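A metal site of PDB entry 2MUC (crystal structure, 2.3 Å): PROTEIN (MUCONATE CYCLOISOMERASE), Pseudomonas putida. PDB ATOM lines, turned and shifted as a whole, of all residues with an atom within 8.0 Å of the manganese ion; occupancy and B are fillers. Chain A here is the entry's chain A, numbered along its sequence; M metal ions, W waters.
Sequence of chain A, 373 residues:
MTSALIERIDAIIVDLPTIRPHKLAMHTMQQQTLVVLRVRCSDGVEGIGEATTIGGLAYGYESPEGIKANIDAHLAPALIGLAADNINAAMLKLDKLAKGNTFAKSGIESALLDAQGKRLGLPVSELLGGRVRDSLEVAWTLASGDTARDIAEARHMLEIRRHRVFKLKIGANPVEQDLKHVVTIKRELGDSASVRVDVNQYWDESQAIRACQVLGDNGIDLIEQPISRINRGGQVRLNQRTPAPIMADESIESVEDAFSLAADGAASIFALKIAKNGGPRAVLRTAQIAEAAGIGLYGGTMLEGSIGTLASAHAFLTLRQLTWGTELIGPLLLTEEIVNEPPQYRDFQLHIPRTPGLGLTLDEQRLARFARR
The manganese ion is bound by water W2, at 2.3 Å. The manganese ion is bound by the side-chain carboxylate (OD2) of Asp 249, at 2.4 Å. The manganese ion is bound by water W3, at 2.4 Å. Water W1 binds the manganese ion. The side-chain carboxylate (OE2) of Glu 224 is bound to the manganese ion. The manganese ion is bound by OD2 of Asp 198 (2.6 Å). The manganese ion has six donor atoms within binding distance.
The side-chain carboxylate of Glu 327 is in salt-bridge range of the side-chain amino group of Lys 167, at 2.6 Å. The side-chain carboxylate (OD2) of Asp 198 lies close to the side-chain amino group (NZ) of Lys 167. The side-chain carboxylate (OD1) of Asp 249 is in salt-bridge range of the side-chain amino group (NZ) of Lys 273 (3.3 Å). OE1 of Glu 224 is in salt-bridge range of NZ of Lys 167 (2.9 Å). The backbone NH of Asp 249 lies within hydrogen-bond range of the side-chain amide oxygen of Gln 225. The side-chain carboxylate of Asp 198 sits at hydrogen-bond distance from the backbone NH of Asn 200 (3.1 Å). The backbone carbonyl oxygen (O) of Glu 224 sits at hydrogen-bond distance from the backbone NH (N) of Val 199, 3.0 Å away. The backbone carbonyl oxygen of Val 197 lies within hydrogen-bond range of the backbone NH of Glu 224 (2.8 Å).
Water W3 bridges the side-chain carboxylate (OD1) of Asp 198 and the side-chain carboxylate (OE1) of Glu 250. Water W1 lies within hydrogen-bond range of NZ of Lys 167 (3.0 Å), OE2 of Glu 327 (3.2 Å) and NZ of Lys 273 (3.3 Å). Water W2 lies within hydrogen-bond range of OD1 of Asn 200 (2.7 Å) and OE2 of Glu 250 (2.9 Å).
Merely in contact with the manganese ion: Lys 167 (3.9 Å). Within 4 Å of the manganese ion: Lys 167, Asp 198, Glu 224 and Asp 249.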
ATOM      1  N   ILE A  54     -16.090 -17.218 -12.104  1.00  0.00           N
ATOM      2  CA  ILE A  54     -16.489 -17.506 -13.474  1.00  0.00           C
ATOM      3  C   ILE A  54     -17.342 -16.361 -14.016  1.00  0.00           C
ATOM      4  O   ILE A  54     -18.270 -15.918 -13.351  1.00  0.00           O
ATOM      5  CB  ILE A  54     -17.342 -18.772 -13.555  1.00  0.00           C
ATOM      6  CG1 ILE A  54     -16.636 -19.923 -12.864  1.00  0.00           C
ATOM      7  CG2 ILE A  54     -17.642 -19.120 -14.998  1.00  0.00           C
ATOM      8  CD1 ILE A  54     -17.576 -21.060 -12.558  1.00  0.00           C
ATOM      9  N   TYR A  59     -21.511 -14.959 -11.628  1.00  0.00           N
ATOM     10  CA  TYR A  59     -21.704 -16.068 -10.681  1.00  0.00           C
ATOM     11  C   TYR A  59     -21.274 -15.691  -9.258  1.00  0.00           C
ATOM     12  O   TYR A  59     -21.078 -16.564  -8.397  1.00  0.00           O
ATOM     13  CB  TYR A  59     -20.945 -17.317 -11.154  1.00  0.00           C
ATOM     14  CG  TYR A  59     -21.386 -17.857 -12.497  1.00  0.00           C
ATOM     15  CD1 TYR A  59     -20.917 -17.303 -13.690  1.00  0.00           C
ATOM     16  CD2 TYR A  59     -22.270 -18.935 -12.596  1.00  0.00           C
ATOM     17  CE1 TYR A  59     -21.318 -17.791 -14.949  1.00  0.00           C
ATOM     18  CE2 TYR A  59     -22.685 -19.433 -13.859  1.00  0.00           C
ATOM     19  CZ  TYR A  59     -22.192 -18.860 -15.030  1.00  0.00           C
ATOM     20  OH  TYR A  59     -22.596 -19.334 -16.260  1.00  0.00           O
ATOM     21  N   LYS A 167     -21.454 -34.434 -14.709  1.00  0.00           N
ATOM     22  CA  LYS A 167     -22.352 -33.365 -14.350  1.00  0.00           C
ATOM     23  C   LYS A 167     -22.779 -32.608 -15.604  1.00  0.00           C
ATOM     24  O   LYS A 167     -21.965 -32.364 -16.500  1.00  0.00           O
ATOM     25  CB  LYS A 167     -21.635 -32.442 -13.377  1.00  0.00           C
ATOM     26  CG  LYS A 167     -22.405 -31.250 -12.907  1.00  0.00           C
ATOM     27  CD  LYS A 167     -21.610 -30.556 -11.828  1.00  0.00           C
ATOM     28  CE  LYS A 167     -21.938 -29.093 -11.760  1.00  0.00           C
ATOM     29  NZ  LYS A 167     -21.418 -28.448 -10.542  1.00  0.00           N
ATOM     30  N   LYS A 169     -24.725 -29.104 -16.954  1.00  0.00           N
ATOM     31  CA  LYS A 169     -25.245 -27.758 -16.662  1.00  0.00           C
ATOM     32  C   LYS A 169     -26.485 -27.559 -17.518  1.00  0.00           C
ATOM     33  O   LYS A 169     -26.405 -27.531 -18.756  1.00  0.00           O
ATOM     34  CB  LYS A 169     -24.245 -26.653 -17.023  1.00  0.00           C
ATOM     35  CG  LYS A 169     -23.052 -26.514 -16.117  1.00  0.00           C
ATOM     36  CD  LYS A 169     -22.128 -25.397 -16.618  1.00  0.00           C
ATOM     37  CE  LYS A 169     -20.854 -25.333 -15.784  1.00  0.00           C
ATOM     38  NZ  LYS A 169     -19.844 -24.338 -16.288  1.00  0.00           N
ATOM     39  N   VAL A 197     -27.044 -33.155 -12.262  1.00  0.00           N
ATOM     40  CA  VAL A 197     -27.289 -31.927 -13.008  1.00  0.00           C
ATOM     41  C   VAL A 197     -27.082 -30.746 -12.116  1.00  0.00           C
ATOM     42  O   VAL A 197     -27.134 -30.852 -10.891  1.00  0.00           O
ATOM     43  CB  VAL A 197     -28.707 -31.839 -13.607  1.00  0.00           C
ATOM     44  CG1 VAL A 197     -28.841 -32.815 -14.767  1.00  0.00           C
ATOM     45  CG2 VAL A 197     -29.764 -32.123 -12.554  1.00  0.00           C
ATOM     46  N   ASP A 198     -26.860 -29.605 -12.745  1.00  0.00           N
ATOM     47  CA  ASP A 198     -26.667 -28.360 -12.056  1.00  0.00           C
ATOM     48  C   ASP A 198     -27.507 -27.369 -12.851  1.00  0.00           C
ATOM     49  O   ASP A 198     -27.239 -27.136 -14.028  1.00  0.00           O
ATOM     50  CB  ASP A 198     -25.202 -27.985 -12.074  1.00  0.00           C
ATOM     51  CG  ASP A 198     -24.893 -26.778 -11.225  1.00  0.00           C
ATOM     52  OD1 ASP A 198     -25.816 -26.064 -10.774  1.00  0.00           O
ATOM     53  OD2 ASP A 198     -23.693 -26.525 -11.011  1.00  0.00           O
ATOM     54  N   VAL A 199     -28.540 -26.816 -12.211  1.00  0.00           N
ATOM     55  CA  VAL A 199     -29.426 -25.857 -12.894  1.00  0.00           C
ATOM     56  C   VAL A 199     -29.041 -24.390 -12.696  1.00  0.00           C
ATOM     57  O   VAL A 199     -29.696 -23.494 -13.229  1.00  0.00           O
ATOM     58  CB  VAL A 199     -30.891 -26.058 -12.494  1.00  0.00           C
ATOM     59  CG1 VAL A 199     -31.797 -25.498 -13.571  1.00  0.00           C
ATOM     60  CG2 VAL A 199     -31.181 -27.541 -12.281  1.00  0.00           C
ATOM     61  N   ASN A 200     -28.036 -24.166 -11.868  1.00  0.00           N
ATOM     62  CA  ASN A 200     -27.515 -22.834 -11.599  1.00  0.00           C
ATOM     63  C   ASN A 200     -28.573 -21.777 -11.353  1.00  0.00           C
ATOM     64  O   ASN A 200     -28.488 -20.685 -11.890  1.00  0.00           O
ATOM     65  CB  ASN A 200     -26.560 -22.421 -12.735  1.00  0.00           C
ATOM     66  CG  ASN A 200     -25.228 -23.162 -12.688  1.00  0.00           C
ATOM     67  OD1 ASN A 200     -24.359 -22.848 -11.880  1.00  0.00           O
ATOM     68  ND2 ASN A 200     -25.097 -24.219 -13.496  1.00  0.00           N
ATOM     69  N   GLN A 201     -29.544 -22.123 -10.518  1.00  0.00           N
ATOM     70  CA  GLN A 201     -30.639 -21.208 -10.156  1.00  0.00           C
ATOM     71  C   GLN A 201     -31.548 -20.805 -11.322  1.00  0.00           C
ATOM     72  O   GLN A 201     -32.377 -19.914 -11.169  1.00  0.00           O
ATOM     73  CB  GLN A 201     -30.070 -19.907  -9.526  1.00  0.00           C
ATOM     74  CG  GLN A 201     -29.106 -20.112  -8.353  1.00  0.00           C
ATOM     75  CD  GLN A 201     -28.825 -18.824  -7.601  1.00  0.00           C
ATOM     76  OE1 GLN A 201     -29.454 -18.543  -6.581  1.00  0.00           O
ATOM     77  NE2 GLN A 201     -27.875 -18.050  -8.093  1.00  0.00           N
ATOM     78  N   GLU A 224     -28.433 -30.269  -8.464  1.00  0.00           N
ATOM     79  CA  GLU A 224     -27.762 -29.168  -7.809  1.00  0.00           C
ATOM     80  C   GLU A 224     -28.395 -27.799  -8.081  1.00  0.00           C
ATOM     81  O   GLU A 224     -28.642 -27.432  -9.227  1.00  0.00           O
ATOM     82  CB  GLU A 224     -26.305 -29.186  -8.254  1.00  0.00           C
ATOM     83  CG  GLU A 224     -25.433 -28.084  -7.745  1.00  0.00           C
ATOM     84  CD  GLU A 224     -23.993 -28.282  -8.150  1.00  0.00           C
ATOM     85  OE1 GLU A 224     -23.691 -29.167  -8.961  1.00  0.00           O
ATOM     86  OE2 GLU A 224     -23.118 -27.577  -7.623  1.00  0.00           O
ATOM     87  N   GLN A 225     -28.615 -27.047  -7.009  1.00  0.00           N
ATOM     88  CA  GLN A 225     -29.222 -25.705  -7.030  1.00  0.00           C
ATOM     89  C   GLN A 225     -30.290 -25.494  -8.109  1.00  0.00           C
ATOM     90  O   GLN A 225     -30.171 -24.567  -8.943  1.00  0.00           O
ATOM     91  CB  GLN A 225     -28.157 -24.625  -7.158  1.00  0.00           C
ATOM     92  CG  GLN A 225     -28.665 -23.230  -6.803  1.00  0.00           C
ATOM     93  CD  GLN A 225     -28.731 -23.033  -5.312  1.00  0.00           C
ATOM     94  OE1 GLN A 225     -27.883 -23.521  -4.578  1.00  0.00           O
ATOM     95  NE2 GLN A 225     -29.733 -22.291  -4.856  1.00  0.00           N
ATOM     96  N   MET A 247     -28.997 -30.445  -3.724  1.00  0.00           N
ATOM     97  CA  MET A 247     -27.726 -29.929  -3.241  1.00  0.00           C
ATOM     98  C   MET A 247     -27.698 -28.402  -3.304  1.00  0.00           C
ATOM     99  O   MET A 247     -28.095 -27.813  -4.289  1.00  0.00           O
ATOM    100  CB  MET A 247     -26.566 -30.495  -4.065  1.00  0.00           C
ATOM    101  CG  MET A 247     -25.199 -29.907  -3.730  1.00  0.00           C
ATOM    102  SD  MET A 247     -23.816 -30.787  -4.449  1.00  0.00           S
ATOM    103  CE  MET A 247     -23.370 -29.762  -5.645  1.00  0.00           C
ATOM    104  N   ALA A 248     -27.220 -27.779  -2.237  1.00  0.00           N
ATOM    105  CA  ALA A 248     -27.142 -26.331  -2.233  1.00  0.00           C
ATOM    106  C   ALA A 248     -25.755 -25.864  -2.651  1.00  0.00           C
ATOM    107  O   ALA A 248     -24.741 -26.443  -2.220  1.00  0.00           O
ATOM    108  CB  ALA A 248     -27.489 -25.782  -0.865  1.00  0.00           C
ATOM    109  N   ASP A 249     -25.718 -24.844  -3.497  1.00  0.00           N
ATOM    110  CA  ASP A 249     -24.453 -24.246  -3.930  1.00  0.00           C
ATOM    111  C   ASP A 249     -24.517 -22.747  -3.762  1.00  0.00           C
ATOM    112  O   ASP A 249     -23.942 -22.201  -2.821  1.00  0.00           O
ATOM    113  CB  ASP A 249     -24.085 -24.576  -5.375  1.00  0.00           C
ATOM    114  CG  ASP A 249     -22.770 -23.953  -5.793  1.00  0.00           C
ATOM    115  OD1 ASP A 249     -22.185 -23.107  -5.081  1.00  0.00           O
ATOM    116  OD2 ASP A 249     -22.283 -24.313  -6.856  1.00  0.00           O
ATOM    117  N   GLU A 250     -25.204 -22.080  -4.679  1.00  0.00           N
ATOM    118  CA  GLU A 250     -25.326 -20.616  -4.624  1.00  0.00           C
ATOM    119  C   GLU A 250     -25.977 -20.101  -3.368  1.00  0.00           C
ATOM    120  O   GLU A 250     -25.779 -18.947  -3.001  1.00  0.00           O
ATOM    121  CB  GLU A 250     -26.066 -20.051  -5.836  1.00  0.00           C
ATOM    122  CG  GLU A 250     -25.204 -19.911  -7.071  1.00  0.00           C
ATOM    123  CD  GLU A 250     -24.911 -21.230  -7.763  1.00  0.00           C
ATOM    124  OE1 GLU A 250     -25.718 -22.184  -7.656  1.00  0.00           O
ATOM    125  OE2 GLU A 250     -23.851 -21.307  -8.414  1.00  0.00           O
ATOM    126  N   ALA A 271     -22.577 -27.976  -1.234  1.00  0.00           N
ATOM    127  CA  ALA A 271     -21.413 -27.912  -2.084  1.00  0.00           C
ATOM    128  C   ALA A 271     -20.425 -27.051  -1.274  1.00  0.00           C
ATOM    129  O   ALA A 271     -20.826 -26.009  -0.745  1.00  0.00           O
ATOM    130  CB  ALA A 271     -21.737 -27.225  -3.403  1.00  0.00           C
ATOM    131  N   LYS A 273     -17.233 -24.701  -1.238  1.00  0.00           N
ATOM    132  CA  LYS A 273     -16.363 -23.942  -2.114  1.00  0.00           C
ATOM    133  C   LYS A 273     -15.573 -22.971  -1.283  1.00  0.00           C
ATOM    134  O   LYS A 273     -16.153 -22.111  -0.621  1.00  0.00           O
ATOM    135  CB  LYS A 273     -17.168 -23.171  -3.171  1.00  0.00           C
ATOM    136  CG  LYS A 273     -17.902 -24.063  -4.156  1.00  0.00           C
ATOM    137  CD  LYS A 273     -18.559 -23.240  -5.228  1.00  0.00           C
ATOM    138  CE  LYS A 273     -19.188 -24.142  -6.278  1.00  0.00           C
ATOM    139  NZ  LYS A 273     -19.794 -23.371  -7.401  1.00  0.00           N
ATOM    140  N   TYR A 298     -19.933 -32.434  -0.805  1.00  0.00           N
ATOM    141  CA  TYR A 298     -19.451 -32.457  -2.181  1.00  0.00           C
ATOM    142  C   TYR A 298     -18.425 -31.346  -2.321  1.00  0.00           C
ATOM    143  O   TYR A 298     -18.684 -30.225  -1.897  1.00  0.00           O
ATOM    144  CB  TYR A 298     -20.617 -32.200  -3.134  1.00  0.00           C
ATOM    145  CG  TYR A 298     -20.251 -32.133  -4.597  1.00  0.00           C
ATOM    146  CD1 TYR A 298     -19.860 -33.267  -5.298  1.00  0.00           C
ATOM    147  CD2 TYR A 298     -20.370 -30.942  -5.291  1.00  0.00           C
ATOM    148  CE1 TYR A 298     -19.627 -33.220  -6.682  1.00  0.00           C
ATOM    149  CE2 TYR A 298     -20.142 -30.884  -6.684  1.00  0.00           C
ATOM    150  CZ  TYR A 298     -19.771 -32.022  -7.354  1.00  0.00           C
ATOM    151  OH  TYR A 298     -19.646 -31.981  -8.726  1.00  0.00           O
ATOM    152  N   GLY A 300     -16.806 -28.630  -4.156  1.00  0.00           N
ATOM    153  CA  GLY A 300     -17.049 -27.785  -5.312  1.00  0.00           C
ATOM    154  C   GLY A 300     -15.862 -26.962  -5.740  1.00  0.00           C
ATOM    155  O   GLY A 300     -14.835 -26.899  -5.053  1.00  0.00           O
ATOM    156  N   THR A 301     -16.028 -26.270  -6.872  1.00  0.00           N
ATOM    157  CA  THR A 301     -14.975 -25.453  -7.422  1.00  0.00           C
ATOM    158  C   THR A 301     -15.562 -24.278  -8.181  1.00  0.00           C
ATOM    159  O   THR A 301     -16.726 -24.292  -8.570  1.00  0.00           O
ATOM    160  CB  THR A 301     -14.114 -26.284  -8.421  1.00  0.00           C
ATOM    161  OG1 THR A 301     -12.987 -25.506  -8.860  1.00  0.00           O
ATOM    162  CG2 THR A 301     -14.933 -26.687  -9.664  1.00  0.00           C
ATOM    163  N   MET A 302     -14.757 -23.224  -8.297  1.00  0.00           N
ATOM    164  CA  MET A 302     -15.130 -22.043  -9.088  1.00  0.00           C
ATOM    165  C   MET A 302     -14.259 -22.047 -10.356  1.00  0.00           C
ATOM    166  O   MET A 302     -13.962 -21.015 -10.933  1.00  0.00           O
ATOM    167  CB  MET A 302     -14.923 -20.762  -8.285  1.00  0.00           C
ATOM    168  CG  MET A 302     -15.945 -20.543  -7.159  1.00  0.00           C
ATOM    169  SD  MET A 302     -17.726 -20.559  -7.657  1.00  0.00           S
ATOM    170  CE  MET A 302     -17.820 -19.145  -8.766  1.00  0.00           C
ATOM    171  N   GLU A 327     -15.519 -31.910  -7.731  1.00  0.00           N
ATOM    172  CA  GLU A 327     -15.478 -31.517  -9.131  1.00  0.00           C
ATOM    173  C   GLU A 327     -14.240 -30.678  -9.375  1.00  0.00           C
ATOM    174  O   GLU A 327     -14.269 -29.713 -10.114  1.00  0.00           O
ATOM    175  CB  GLU A 327     -16.741 -30.750  -9.526  1.00  0.00           C
ATOM    176  CG  GLU A 327     -17.044 -29.595  -8.608  1.00  0.00           C
ATOM    177  CD  GLU A 327     -18.331 -28.911  -8.995  1.00  0.00           C
ATOM    178  OE1 GLU A 327     -19.121 -29.495  -9.756  1.00  0.00           O
ATOM    179  OE2 GLU A 327     -18.543 -27.764  -8.543  1.00  0.00           O
HETATM  180 MN    MN M   1     -23.063 -25.411  -8.782  1.00  0.00          MN
HETATM  181  O   HOH W   1     -20.794 -25.685  -9.516  1.00  0.00           O
HETATM  182  O   HOH W   2     -22.613 -23.472  -9.962  1.00  0.00           O
HETATM  183  O   HOH W   3     -25.309 -24.673  -8.584  1.00  0.00           O
HETATM  184  O   HOH W   4     -20.727 -26.889  -6.727  1.00  0.00           O
